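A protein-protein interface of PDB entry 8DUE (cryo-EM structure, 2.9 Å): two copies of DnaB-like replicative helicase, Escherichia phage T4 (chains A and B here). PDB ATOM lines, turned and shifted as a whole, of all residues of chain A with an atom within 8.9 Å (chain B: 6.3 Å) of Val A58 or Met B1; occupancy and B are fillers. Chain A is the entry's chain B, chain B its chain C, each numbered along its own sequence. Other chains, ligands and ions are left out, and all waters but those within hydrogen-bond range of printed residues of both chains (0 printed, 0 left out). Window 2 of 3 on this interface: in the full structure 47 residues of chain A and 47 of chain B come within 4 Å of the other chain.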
ATOM      1  N   LEU A  39      -4.277  -7.081 -15.216  1.00  0.00           N
ATOM      2  CA  LEU A  39      -5.607  -7.484 -15.665  1.00  0.00           C
ATOM      3  C   LEU A  39      -6.549  -6.289 -15.711  1.00  0.00           C
ATOM      4  O   LEU A  39      -7.309  -6.118 -16.675  1.00  0.00           O
ATOM      5  CB  LEU A  39      -6.172  -8.566 -14.746  1.00  0.00           C
ATOM      6  CG  LEU A  39      -5.384  -9.866 -14.604  1.00  0.00           C
ATOM      7  CD1 LEU A  39      -6.097 -10.816 -13.655  1.00  0.00           C
ATOM      8  CD2 LEU A  39      -5.169 -10.514 -15.959  1.00  0.00           C
ATOM      9  N   HIS A  43      -8.401  -4.735 -19.039  1.00  0.00           N
ATOM     10  CA  HIS A  43      -9.851  -4.592 -19.132  1.00  0.00           C
ATOM     11  C   HIS A  43     -10.247  -3.148 -19.419  1.00  0.00           C
ATOM     12  O   HIS A  43     -11.105  -2.887 -20.269  1.00  0.00           O
ATOM     13  CB  HIS A  43     -10.516  -5.087 -17.850  1.00  0.00           C
ATOM     14  CG  HIS A  43     -12.001  -5.226 -17.962  1.00  0.00           C
ATOM     15  ND1 HIS A  43     -12.854  -4.145 -17.946  1.00  0.00           N
ATOM     16  CD2 HIS A  43     -12.786  -6.322 -18.092  1.00  0.00           C
ATOM     17  CE1 HIS A  43     -14.100  -4.566 -18.063  1.00  0.00           C
ATOM     18  NE2 HIS A  43     -14.087  -5.884 -18.153  1.00  0.00           N
ATOM     19  N   SER A  52     -15.834  -5.255 -13.311  1.00  0.00           N
ATOM     20  CA  SER A  52     -16.461  -5.777 -12.112  1.00  0.00           C
ATOM     21  C   SER A  52     -15.616  -6.911 -11.540  1.00  0.00           C
ATOM     22  O   SER A  52     -14.616  -7.333 -12.125  1.00  0.00           O
ATOM     23  CB  SER A  52     -17.879  -6.261 -12.412  1.00  0.00           C
ATOM     24  OG  SER A  52     -18.670  -5.217 -12.952  1.00  0.00           O
ATOM     25  N   ILE A  53     -16.024  -7.404 -10.369  1.00  0.00           N
ATOM     26  CA  ILE A  53     -15.328  -8.541  -9.779  1.00  0.00           C
ATOM     27  C   ILE A  53     -15.468  -9.767 -10.672  1.00  0.00           C
ATOM     28  O   ILE A  53     -14.498 -10.500 -10.905  1.00  0.00           O
ATOM     29  CB  ILE A  53     -15.842  -8.805  -8.350  1.00  0.00           C
ATOM     30  CG1 ILE A  53     -15.247 -10.102  -7.797  1.00  0.00           C
ATOM     31  CG2 ILE A  53     -17.365  -8.833  -8.313  1.00  0.00           C
ATOM     32  CD1 ILE A  53     -15.627 -10.377  -6.363  1.00  0.00           C
ATOM     33  N   ASN A  54     -16.675 -10.007 -11.193  1.00  0.00           N
ATOM     34  CA  ASN A  54     -16.875 -11.110 -12.128  1.00  0.00           C
ATOM     35  C   ASN A  54     -16.079 -10.898 -13.407  1.00  0.00           C
ATOM     36  O   ASN A  54     -15.435 -11.826 -13.907  1.00  0.00           O
ATOM     37  CB  ASN A  54     -18.359 -11.271 -12.444  1.00  0.00           C
ATOM     38  CG  ASN A  54     -19.146 -11.811 -11.272  1.00  0.00           C
ATOM     39  OD1 ASN A  54     -18.636 -12.601 -10.480  1.00  0.00           O
ATOM     40  ND2 ASN A  54     -20.398 -11.387 -11.154  1.00  0.00           N
ATOM     41  N   ALA A  55     -16.101  -9.679 -13.948  1.00  0.00           N
ATOM     42  CA  ALA A  55     -15.340  -9.383 -15.154  1.00  0.00           C
ATOM     43  C   ALA A  55     -13.841  -9.516 -14.948  1.00  0.00           C
ATOM     44  O   ALA A  55     -13.100  -9.591 -15.934  1.00  0.00           O
ATOM     45  CB  ALA A  55     -15.666  -7.975 -15.652  1.00  0.00           C
ATOM     46  N   LEU A  56     -13.379  -9.542 -13.700  1.00  0.00           N
ATOM     47  CA  LEU A  56     -11.965  -9.662 -13.383  1.00  0.00           C
ATOM     48  C   LEU A  56     -11.548 -11.104 -13.123  1.00  0.00           C
ATOM     49  O   LEU A  56     -10.578 -11.584 -13.714  1.00  0.00           O
ATOM     50  CB  LEU A  56     -11.631  -8.787 -12.168  1.00  0.00           C
ATOM     51  CG  LEU A  56     -10.157  -8.622 -11.804  1.00  0.00           C
ATOM     52  CD1 LEU A  56      -9.357  -8.234 -13.031  1.00  0.00           C
ATOM     53  CD2 LEU A  56      -9.994  -7.579 -10.709  1.00  0.00           C
ATOM     54  N   ASN A  57     -12.264 -11.805 -12.246  1.00  0.00           N
ATOM     55  CA  ASN A  57     -11.857 -13.142 -11.837  1.00  0.00           C
ATOM     56  C   ASN A  57     -12.412 -14.250 -12.724  1.00  0.00           C
ATOM     57  O   ASN A  57     -12.034 -15.411 -12.539  1.00  0.00           O
ATOM     58  CB  ASN A  57     -12.274 -13.401 -10.385  1.00  0.00           C
ATOM     59  CG  ASN A  57     -13.750 -13.697 -10.244  1.00  0.00           C
ATOM     60  OD1 ASN A  57     -14.572 -13.200 -11.011  1.00  0.00           O
ATOM     61  ND2 ASN A  57     -14.096 -14.514  -9.257  1.00  0.00           N
ATOM     62  N   VAL A  58     -13.293 -13.935 -13.671  1.00  0.00           N
ATOM     63  CA  VAL A  58     -13.887 -14.971 -14.510  1.00  0.00           C
ATOM     64  C   VAL A  58     -13.419 -14.809 -15.949  1.00  0.00           C
ATOM     65  O   VAL A  58     -12.785 -15.710 -16.510  1.00  0.00           O
ATOM     66  CB  VAL A  58     -15.422 -14.948 -14.428  1.00  0.00           C
ATOM     67  CG1 VAL A  58     -16.012 -15.926 -15.421  1.00  0.00           C
ATOM     68  CG2 VAL A  58     -15.880 -15.283 -13.019  1.00  0.00           C
ATOM     69  N   ALA A  59     -13.736 -13.666 -16.563  1.00  0.00           N
ATOM     70  CA  ALA A  59     -13.298 -13.425 -17.933  1.00  0.00           C
ATOM     71  C   ALA A  59     -11.778 -13.404 -18.020  1.00  0.00           C
ATOM     72  O   ALA A  59     -11.178 -14.126 -18.825  1.00  0.00           O
ATOM     73  CB  ALA A  59     -13.887 -12.114 -18.453  1.00  0.00           C
ATOM     74  N   LEU A  60     -11.141 -12.595 -17.187  1.00  0.00           N
ATOM     75  CA  LEU A  60      -9.705 -12.656 -16.997  1.00  0.00           C
ATOM     76  C   LEU A  60      -9.416 -13.623 -15.857  1.00  0.00           C
ATOM     77  O   LEU A  60     -10.290 -14.393 -15.439  1.00  0.00           O
ATOM     78  CB  LEU A  60      -9.134 -11.260 -16.745  1.00  0.00           C
ATOM     79  CG  LEU A  60      -8.586 -10.556 -17.988  1.00  0.00           C
ATOM     80  CD1 LEU A  60      -7.511 -11.408 -18.646  1.00  0.00           C
ATOM     81  CD2 LEU A  60      -9.693 -10.230 -18.980  1.00  0.00           C
ATOM     82  N   GLU A  61      -8.168 -13.619 -15.380  1.00  0.00           N
ATOM     83  CA  GLU A  61      -7.689 -14.521 -14.335  1.00  0.00           C
ATOM     84  C   GLU A  61      -7.542 -15.929 -14.905  1.00  0.00           C
ATOM     85  O   GLU A  61      -7.000 -16.827 -14.253  1.00  0.00           O
ATOM     86  CB  GLU A  61      -8.621 -14.480 -13.113  1.00  0.00           C
ATOM     87  CG  GLU A  61      -8.321 -15.454 -11.986  1.00  0.00           C
ATOM     88  CD  GLU A  61      -7.050 -15.124 -11.233  1.00  0.00           C
ATOM     89  OE1 GLU A  61      -5.969 -15.075 -11.856  1.00  0.00           O
ATOM     90  OE2 GLU A  61      -7.134 -14.914 -10.008  1.00  0.00           O
ATOM     91  N   ASN A  62      -7.976 -16.116 -16.151  1.00  0.00           N
ATOM     92  CA  ASN A  62      -7.800 -17.366 -16.877  1.00  0.00           C
ATOM     93  C   ASN A  62      -6.784 -17.214 -18.005  1.00  0.00           C
ATOM     94  O   ASN A  62      -6.909 -17.846 -19.056  1.00  0.00           O
ATOM     95  CB  ASN A  62      -9.137 -17.864 -17.423  1.00  0.00           C
ATOM     96  CG  ASN A  62     -10.115 -18.225 -16.323  1.00  0.00           C
ATOM     97  OD1 ASN A  62      -9.922 -17.870 -15.161  1.00  0.00           O
ATOM     98  ND2 ASN A  62     -11.177 -18.933 -16.686  1.00  0.00           N
ATOM     99  N   SER A  63      -5.774 -16.376 -17.794  1.00  0.00           N
ATOM    100  CA  SER A  63      -4.707 -16.181 -18.761  1.00  0.00           C
ATOM    101  C   SER A  63      -3.576 -17.163 -18.463  1.00  0.00           C
ATOM    102  O   SER A  63      -3.716 -18.079 -17.649  1.00  0.00           O
ATOM    103  CB  SER A  63      -4.230 -14.731 -18.738  1.00  0.00           C
ATOM    104  OG  SER A  63      -3.181 -14.528 -19.668  1.00  0.00           O
ATOM    105  N   TYR A  70      -1.103 -17.587  -9.871  1.00  0.00           N
ATOM    106  CA  TYR A  70      -2.543 -17.581 -10.106  1.00  0.00           C
ATOM    107  C   TYR A  70      -3.314 -17.728  -8.799  1.00  0.00           C
ATOM    108  O   TYR A  70      -4.328 -17.050  -8.583  1.00  0.00           O
ATOM    109  CB  TYR A  70      -2.908 -18.692 -11.090  1.00  0.00           C
ATOM    110  CG  TYR A  70      -4.363 -19.091 -11.096  1.00  0.00           C
ATOM    111  CD1 TYR A  70      -5.341 -18.225 -11.561  1.00  0.00           C
ATOM    112  CD2 TYR A  70      -4.757 -20.347 -10.657  1.00  0.00           C
ATOM    113  CE1 TYR A  70      -6.671 -18.592 -11.573  1.00  0.00           C
ATOM    114  CE2 TYR A  70      -6.083 -20.723 -10.668  1.00  0.00           C
ATOM    115  CZ  TYR A  70      -7.035 -19.842 -11.125  1.00  0.00           C
ATOM    116  OH  TYR A  70      -8.358 -20.216 -11.136  1.00  0.00           O
ATOM    117  N   ILE A  77      -7.977 -11.195  -5.236  1.00  0.00           N
ATOM    118  CA  ILE A  77      -9.305 -10.830  -5.724  1.00  0.00           C
ATOM    119  C   ILE A  77     -10.363 -11.170  -4.685  1.00  0.00           C
ATOM    120  O   ILE A  77     -11.341 -10.432  -4.509  1.00  0.00           O
ATOM    121  CB  ILE A  77      -9.590 -11.516  -7.073  1.00  0.00           C
ATOM    122  CG1 ILE A  77      -8.560 -11.086  -8.117  1.00  0.00           C
ATOM    123  CG2 ILE A  77     -10.993 -11.186  -7.557  1.00  0.00           C
ATOM    124  CD1 ILE A  77      -8.381  -9.595  -8.211  1.00  0.00           C
ATOM    125  N   MET B   1     -17.434 -19.039 -17.645  1.00  0.00           N
ATOM    126  CA  MET B   1     -18.380 -17.957 -17.402  1.00  0.00           C
ATOM    127  C   MET B   1     -19.811 -18.414 -17.646  1.00  0.00           C
ATOM    128  O   MET B   1     -20.608 -17.696 -18.244  1.00  0.00           O
ATOM    129  CB  MET B   1     -18.052 -16.751 -18.283  1.00  0.00           C
ATOM    130  CG  MET B   1     -17.846 -17.082 -19.744  1.00  0.00           C
ATOM    131  SD  MET B   1     -17.435 -15.620 -20.707  1.00  0.00           S
ATOM    132  CE  MET B   1     -18.847 -14.579 -20.350  1.00  0.00           C
ATOM    133  N   VAL B   2     -20.127 -19.621 -17.176  1.00  0.00           N
ATOM    134  CA  VAL B   2     -21.483 -20.142 -17.314  1.00  0.00           C
ATOM    135  C   VAL B   2     -22.469 -19.284 -16.535  1.00  0.00           C
ATOM    136  O   VAL B   2     -23.562 -18.965 -17.022  1.00  0.00           O
ATOM    137  CB  VAL B   2     -21.537 -21.611 -16.858  1.00  0.00           C
ATOM    138  CG1 VAL B   2     -22.976 -22.084 -16.781  1.00  0.00           C
ATOM    139  CG2 VAL B   2     -20.731 -22.486 -17.799  1.00  0.00           C
ATOM    140  N   GLU B   3     -22.102 -18.901 -15.311  1.00  0.00           N
ATOM    141  CA  GLU B   3     -23.018 -18.154 -14.456  1.00  0.00           C
ATOM    142  C   GLU B   3     -23.385 -16.815 -15.080  1.00  0.00           C
ATOM    143  O   GLU B   3     -24.556 -16.423 -15.089  1.00  0.00           O
ATOM    144  CB  GLU B   3     -22.393 -17.945 -13.077  1.00  0.00           C
ATOM    145  CG  GLU B   3     -21.798 -19.198 -12.459  1.00  0.00           C
ATOM    146  CD  GLU B   3     -22.848 -20.191 -12.005  1.00  0.00           C
ATOM    147  OE1 GLU B   3     -24.043 -19.827 -11.957  1.00  0.00           O
ATOM    148  OE2 GLU B   3     -22.475 -21.340 -11.691  1.00  0.00           O
ATOM    149  N   ILE B   4     -22.391 -16.102 -15.612  1.00  0.00           N
ATOM    150  CA  ILE B   4     -22.654 -14.801 -16.222  1.00  0.00           C
ATOM    151  C   ILE B   4     -23.575 -14.950 -17.424  1.00  0.00           C
ATOM    152  O   ILE B   4     -24.520 -14.170 -17.603  1.00  0.00           O
ATOM    153  CB  ILE B   4     -21.330 -14.120 -16.607  1.00  0.00           C
ATOM    154  CG1 ILE B   4     -20.503 -13.824 -15.357  1.00  0.00           C
ATOM    155  CG2 ILE B   4     -21.589 -12.847 -17.392  1.00  0.00           C
ATOM    156  CD1 ILE B   4     -19.203 -13.120 -15.648  1.00  0.00           C
ATOM    157  N   ILE B   5     -23.313 -15.951 -18.266  1.00  0.00           N
ATOM    158  CA  ILE B   5     -24.121 -16.151 -19.466  1.00  0.00           C
ATOM    159  C   ILE B   5     -25.561 -16.466 -19.090  1.00  0.00           C
ATOM    160  O   ILE B   5     -26.505 -15.877 -19.630  1.00  0.00           O
ATOM    161  CB  ILE B   5     -23.512 -17.258 -20.343  1.00  0.00           C
ATOM    162  CG1 ILE B   5     -22.172 -16.805 -20.915  1.00  0.00           C
ATOM    163  CG2 ILE B   5     -24.466 -17.637 -21.458  1.00  0.00           C
ATOM    164  CD1 ILE B   5     -21.514 -17.840 -21.782  1.00  0.00           C
ATOM    165  N   LEU B   6     -25.753 -17.394 -18.149  1.00  0.00           N
ATOM    166  CA  LEU B   6     -27.105 -17.747 -17.730  1.00  0.00           C
ATOM    167  C   LEU B   6     -27.820 -16.557 -17.106  1.00  0.00           C
ATOM    168  O   LEU B   6     -28.999 -16.308 -17.394  1.00  0.00           O
ATOM    169  CB  LEU B   6     -27.064 -18.918 -16.751  1.00  0.00           C
ATOM    170  CG  LEU B   6     -26.699 -20.276 -17.349  1.00  0.00           C
ATOM    171  CD1 LEU B   6     -26.671 -21.346 -16.271  1.00  0.00           C
ATOM    172  CD2 LEU B   6     -27.679 -20.643 -18.449  1.00  0.00           C
ATOM    173  N   TYR B  15     -28.774  -8.298 -24.322  1.00  0.00           N
ATOM    174  CA  TYR B  15     -27.871  -9.438 -24.444  1.00  0.00           C
ATOM    175  C   TYR B  15     -28.595 -10.652 -25.010  1.00  0.00           C
ATOM    176  O   TYR B  15     -28.050 -11.372 -25.854  1.00  0.00           O
ATOM    177  CB  TYR B  15     -27.254  -9.759 -23.084  1.00  0.00           C
ATOM    178  CG  TYR B  15     -26.428 -11.023 -23.052  1.00  0.00           C
ATOM    179  CD1 TYR B  15     -25.134 -11.044 -23.552  1.00  0.00           C
ATOM    180  CD2 TYR B  15     -26.936 -12.193 -22.506  1.00  0.00           C
ATOM    181  CE1 TYR B  15     -24.377 -12.194 -23.517  1.00  0.00           C
ATOM    182  CE2 TYR B  15     -26.185 -13.345 -22.466  1.00  0.00           C
ATOM    183  CZ  TYR B  15     -24.907 -13.342 -22.973  1.00  0.00           C
ATOM    184  OH  TYR B  15     -24.158 -14.492 -22.934  1.00  0.00           O
ATOM    185  N   TRP B  89     -18.402  -6.080 -23.699  1.00  0.00           N
ATOM    186  CA  TRP B  89     -17.604  -7.103 -23.037  1.00  0.00           C
ATOM    187  C   TRP B  89     -18.394  -8.395 -22.899  1.00  0.00           C
ATOM    188  O   TRP B  89     -17.847  -9.489 -23.074  1.00  0.00           O
ATOM    189  CB  TRP B  89     -17.142  -6.605 -21.669  1.00  0.00           C
ATOM    190  CG  TRP B  89     -16.598  -7.684 -20.789  1.00  0.00           C
ATOM    191  CD1 TRP B  89     -15.299  -8.076 -20.681  1.00  0.00           C
ATOM    192  CD2 TRP B  89     -17.342  -8.511 -19.890  1.00  0.00           C
ATOM    193  NE1 TRP B  89     -15.186  -9.097 -19.770  1.00  0.00           N
ATOM    194  CE2 TRP B  89     -16.429  -9.384 -19.271  1.00  0.00           C
ATOM    195  CE3 TRP B  89     -18.694  -8.600 -19.549  1.00  0.00           C
ATOM    196  CZ2 TRP B  89     -16.823 -10.332 -18.330  1.00  0.00           C
ATOM    197  CZ3 TRP B  89     -19.083  -9.544 -18.617  1.00  0.00           C
ATOM    198  CH2 TRP B  89     -18.150 -10.396 -18.018  1.00  0.00           C
ATOM    199  N   LEU B  90     -19.687  -8.283 -22.593  1.00  0.00           N
ATOM    200  CA  LEU B  90     -20.525  -9.468 -22.452  1.00  0.00           C
ATOM    201  C   LEU B  90     -20.538 -10.289 -23.733  1.00  0.00           C
ATOM    202  O   LEU B  90     -20.275 -11.496 -23.712  1.00  0.00           O
ATOM    203  CB  LEU B  90     -21.944  -9.059 -22.067  1.00  0.00           C
ATOM    204  CG  LEU B  90     -22.398  -9.449 -20.667  1.00  0.00           C
ATOM    205  CD1 LEU B  90     -23.817  -8.972 -20.446  1.00  0.00           C
ATOM    206  CD2 LEU B  90     -22.296 -10.952 -20.482  1.00  0.00           C
ATOM    207  N   GLU B  93     -16.947 -11.772 -24.620  1.00  0.00           N
ATOM    208  CA  GLU B  93     -16.553 -12.912 -23.803  1.00  0.00           C
ATOM    209  C   GLU B  93     -17.469 -14.104 -24.028  1.00  0.00           C
ATOM    210  O   GLU B  93     -17.018 -15.250 -23.946  1.00  0.00           O
ATOM    211  CB  GLU B  93     -16.527 -12.524 -22.328  1.00  0.00           C
ATOM    212  CG  GLU B  93     -15.542 -11.417 -22.004  1.00  0.00           C
ATOM    213  CD  GLU B  93     -14.100 -11.800 -22.276  1.00  0.00           C
ATOM    214  OE1 GLU B  93     -13.781 -13.007 -22.242  1.00  0.00           O
ATOM    215  OE2 GLU B  93     -13.283 -10.890 -22.524  1.00  0.00           O
ATOM    216  N   THR B  94     -18.749 -13.863 -24.318  1.00  0.00           N
ATOM    217  CA  THR B  94     -19.639 -14.965 -24.660  1.00  0.00           C
ATOM    218  C   THR B  94     -19.206 -15.629 -25.958  1.00  0.00           C
ATOM    219  O   THR B  94     -19.232 -16.859 -26.071  1.00  0.00           O
ATOM    220  CB  THR B  94     -21.077 -14.463 -24.766  1.00  0.00           C
ATOM    221  OG1 THR B  94     -21.471 -13.878 -23.520  1.00  0.00           O
ATOM    222  CG2 THR B  94     -22.011 -15.610 -25.090  1.00  0.00           C
ATOM    223  N   LYS B  96     -16.130 -15.700 -27.080  1.00  0.00           N
ATOM    224  CA  LYS B  96     -14.916 -16.438 -26.744  1.00  0.00           C
ATOM    225  C   LYS B  96     -15.252 -17.770 -26.083  1.00  0.00           C
ATOM    226  O   LYS B  96     -14.690 -18.814 -26.438  1.00  0.00           O
ATOM    227  CB  LYS B  96     -14.029 -15.595 -25.830  1.00  0.00           C
ATOM    228  CG  LYS B  96     -12.784 -16.311 -25.338  1.00  0.00           C
ATOM    229  CD  LYS B  96     -12.071 -15.494 -24.274  1.00  0.00           C
ATOM    230  CE  LYS B  96     -11.672 -14.127 -24.800  1.00  0.00           C
ATOM    231  NZ  LYS B  96     -11.010 -13.313 -23.747  1.00  0.00           N
ATOM    232  N   TYR B  97     -16.173 -17.750 -25.119  1.00  0.00           N
ATOM    233  CA  TYR B  97     -16.554 -18.979 -24.432  1.00  0.00           C
ATOM    234  C   TYR B  97     -17.213 -19.963 -25.386  1.00  0.00           C
ATOM    235  O   TYR B  97     -16.953 -21.170 -25.321  1.00  0.00           O
ATOM    236  CB  TYR B  97     -17.481 -18.663 -23.261  1.00  0.00           C
ATOM    237  CG  TYR B  97     -18.051 -19.888 -22.587  1.00  0.00           C
ATOM    238  CD1 TYR B  97     -17.332 -20.570 -21.617  1.00  0.00           C
ATOM    239  CD2 TYR B  97     -19.311 -20.360 -22.916  1.00  0.00           C
ATOM    240  CE1 TYR B  97     -17.852 -21.689 -20.998  1.00  0.00           C
ATOM    241  CE2 TYR B  97     -19.838 -21.476 -22.303  1.00  0.00           C
ATOM    242  CZ  TYR B  97     -19.106 -22.136 -21.346  1.00  0.00           C
ATOM    243  OH  TYR B  97     -19.632 -23.250 -20.736  1.00  0.00           O
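The backbone carbonyl oxygen (O) of Asn A54 sits close to the side-chain amide oxygen (OD1) of Asn A57 (3.3 Å).
The side-chain amino group (NZ) of Lys B96 is in salt-bridge range of the side-chain carboxylate (OE1) of Glu B93, at 3.2 Å.
Of the printed residues of chain B, His A43 touches Trp B89.
Of the printed residues of chain B, Val A58 touches Met B1 (3.6 Å).
Printed residues of chain B within 4 Å of Ala A59: Trp B89 and Glu B93.
Ser A63 touches none of the printed residues of chain B.
Met B1 touches just one residue of chain A: Val A58.
Printed residues of chain A within 4 Å of Ile B4: Asn A54 (3.8 Å).
Tyr B15 touches none of the printed residues of chain A.
The nearest printed residue of chain B that does not touch Asn A54 is Trp B89 (4.9 Å).
No position is printed for both chains.
NE2 of His A43 touches CD1 of Trp B89, at 3.6 Å.
Asn A54 touches Ile B4 (CB to CD1, 3.8 Å).
Ala A55 touches Trp B89 (CA to CZ2, 3.6 Å).
Val A58 touches Met B1 (CG1 to CB, 3.6 Å).
CZ2 of Trp B89 touches CB of Ala A59, at 3.4 Å.
CD of Glu B93 touches CB of Ala A59 (3.8 Å).
Of the 13 printed residues of chain B, 4 touch a printed residue of chain A.
Printed residues of chain B that touch a printed residue of chain A: Met B1, Ile B4, Trp B89 and Glu B93.
Hydrophobic or aromatic side chains of chain B within 4 Å of the printed part of chain A: Met B1, Ile B4 and Trp B89.
Of the 16 printed residues of chain A, 5 touch a printed residue of chain B.
Printed residues of chain A that touch a printed residue of chain B: His A43, Asn A54, Ala A55, Val A58 and Ala A59.
Hydrophobic or aromatic side chains of chain A within 4 Å of the printed part of chain B: His A43, Ala A55, Val A58 and Ala A59.
Along chain A the printed residues that touch a printed residue of chain B span positions 43 to 59.
Among the printed residues, no Asp or Glu carboxylate lies within 4 Å of a Lys or Arg side-chain nitrogen of the other chain.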
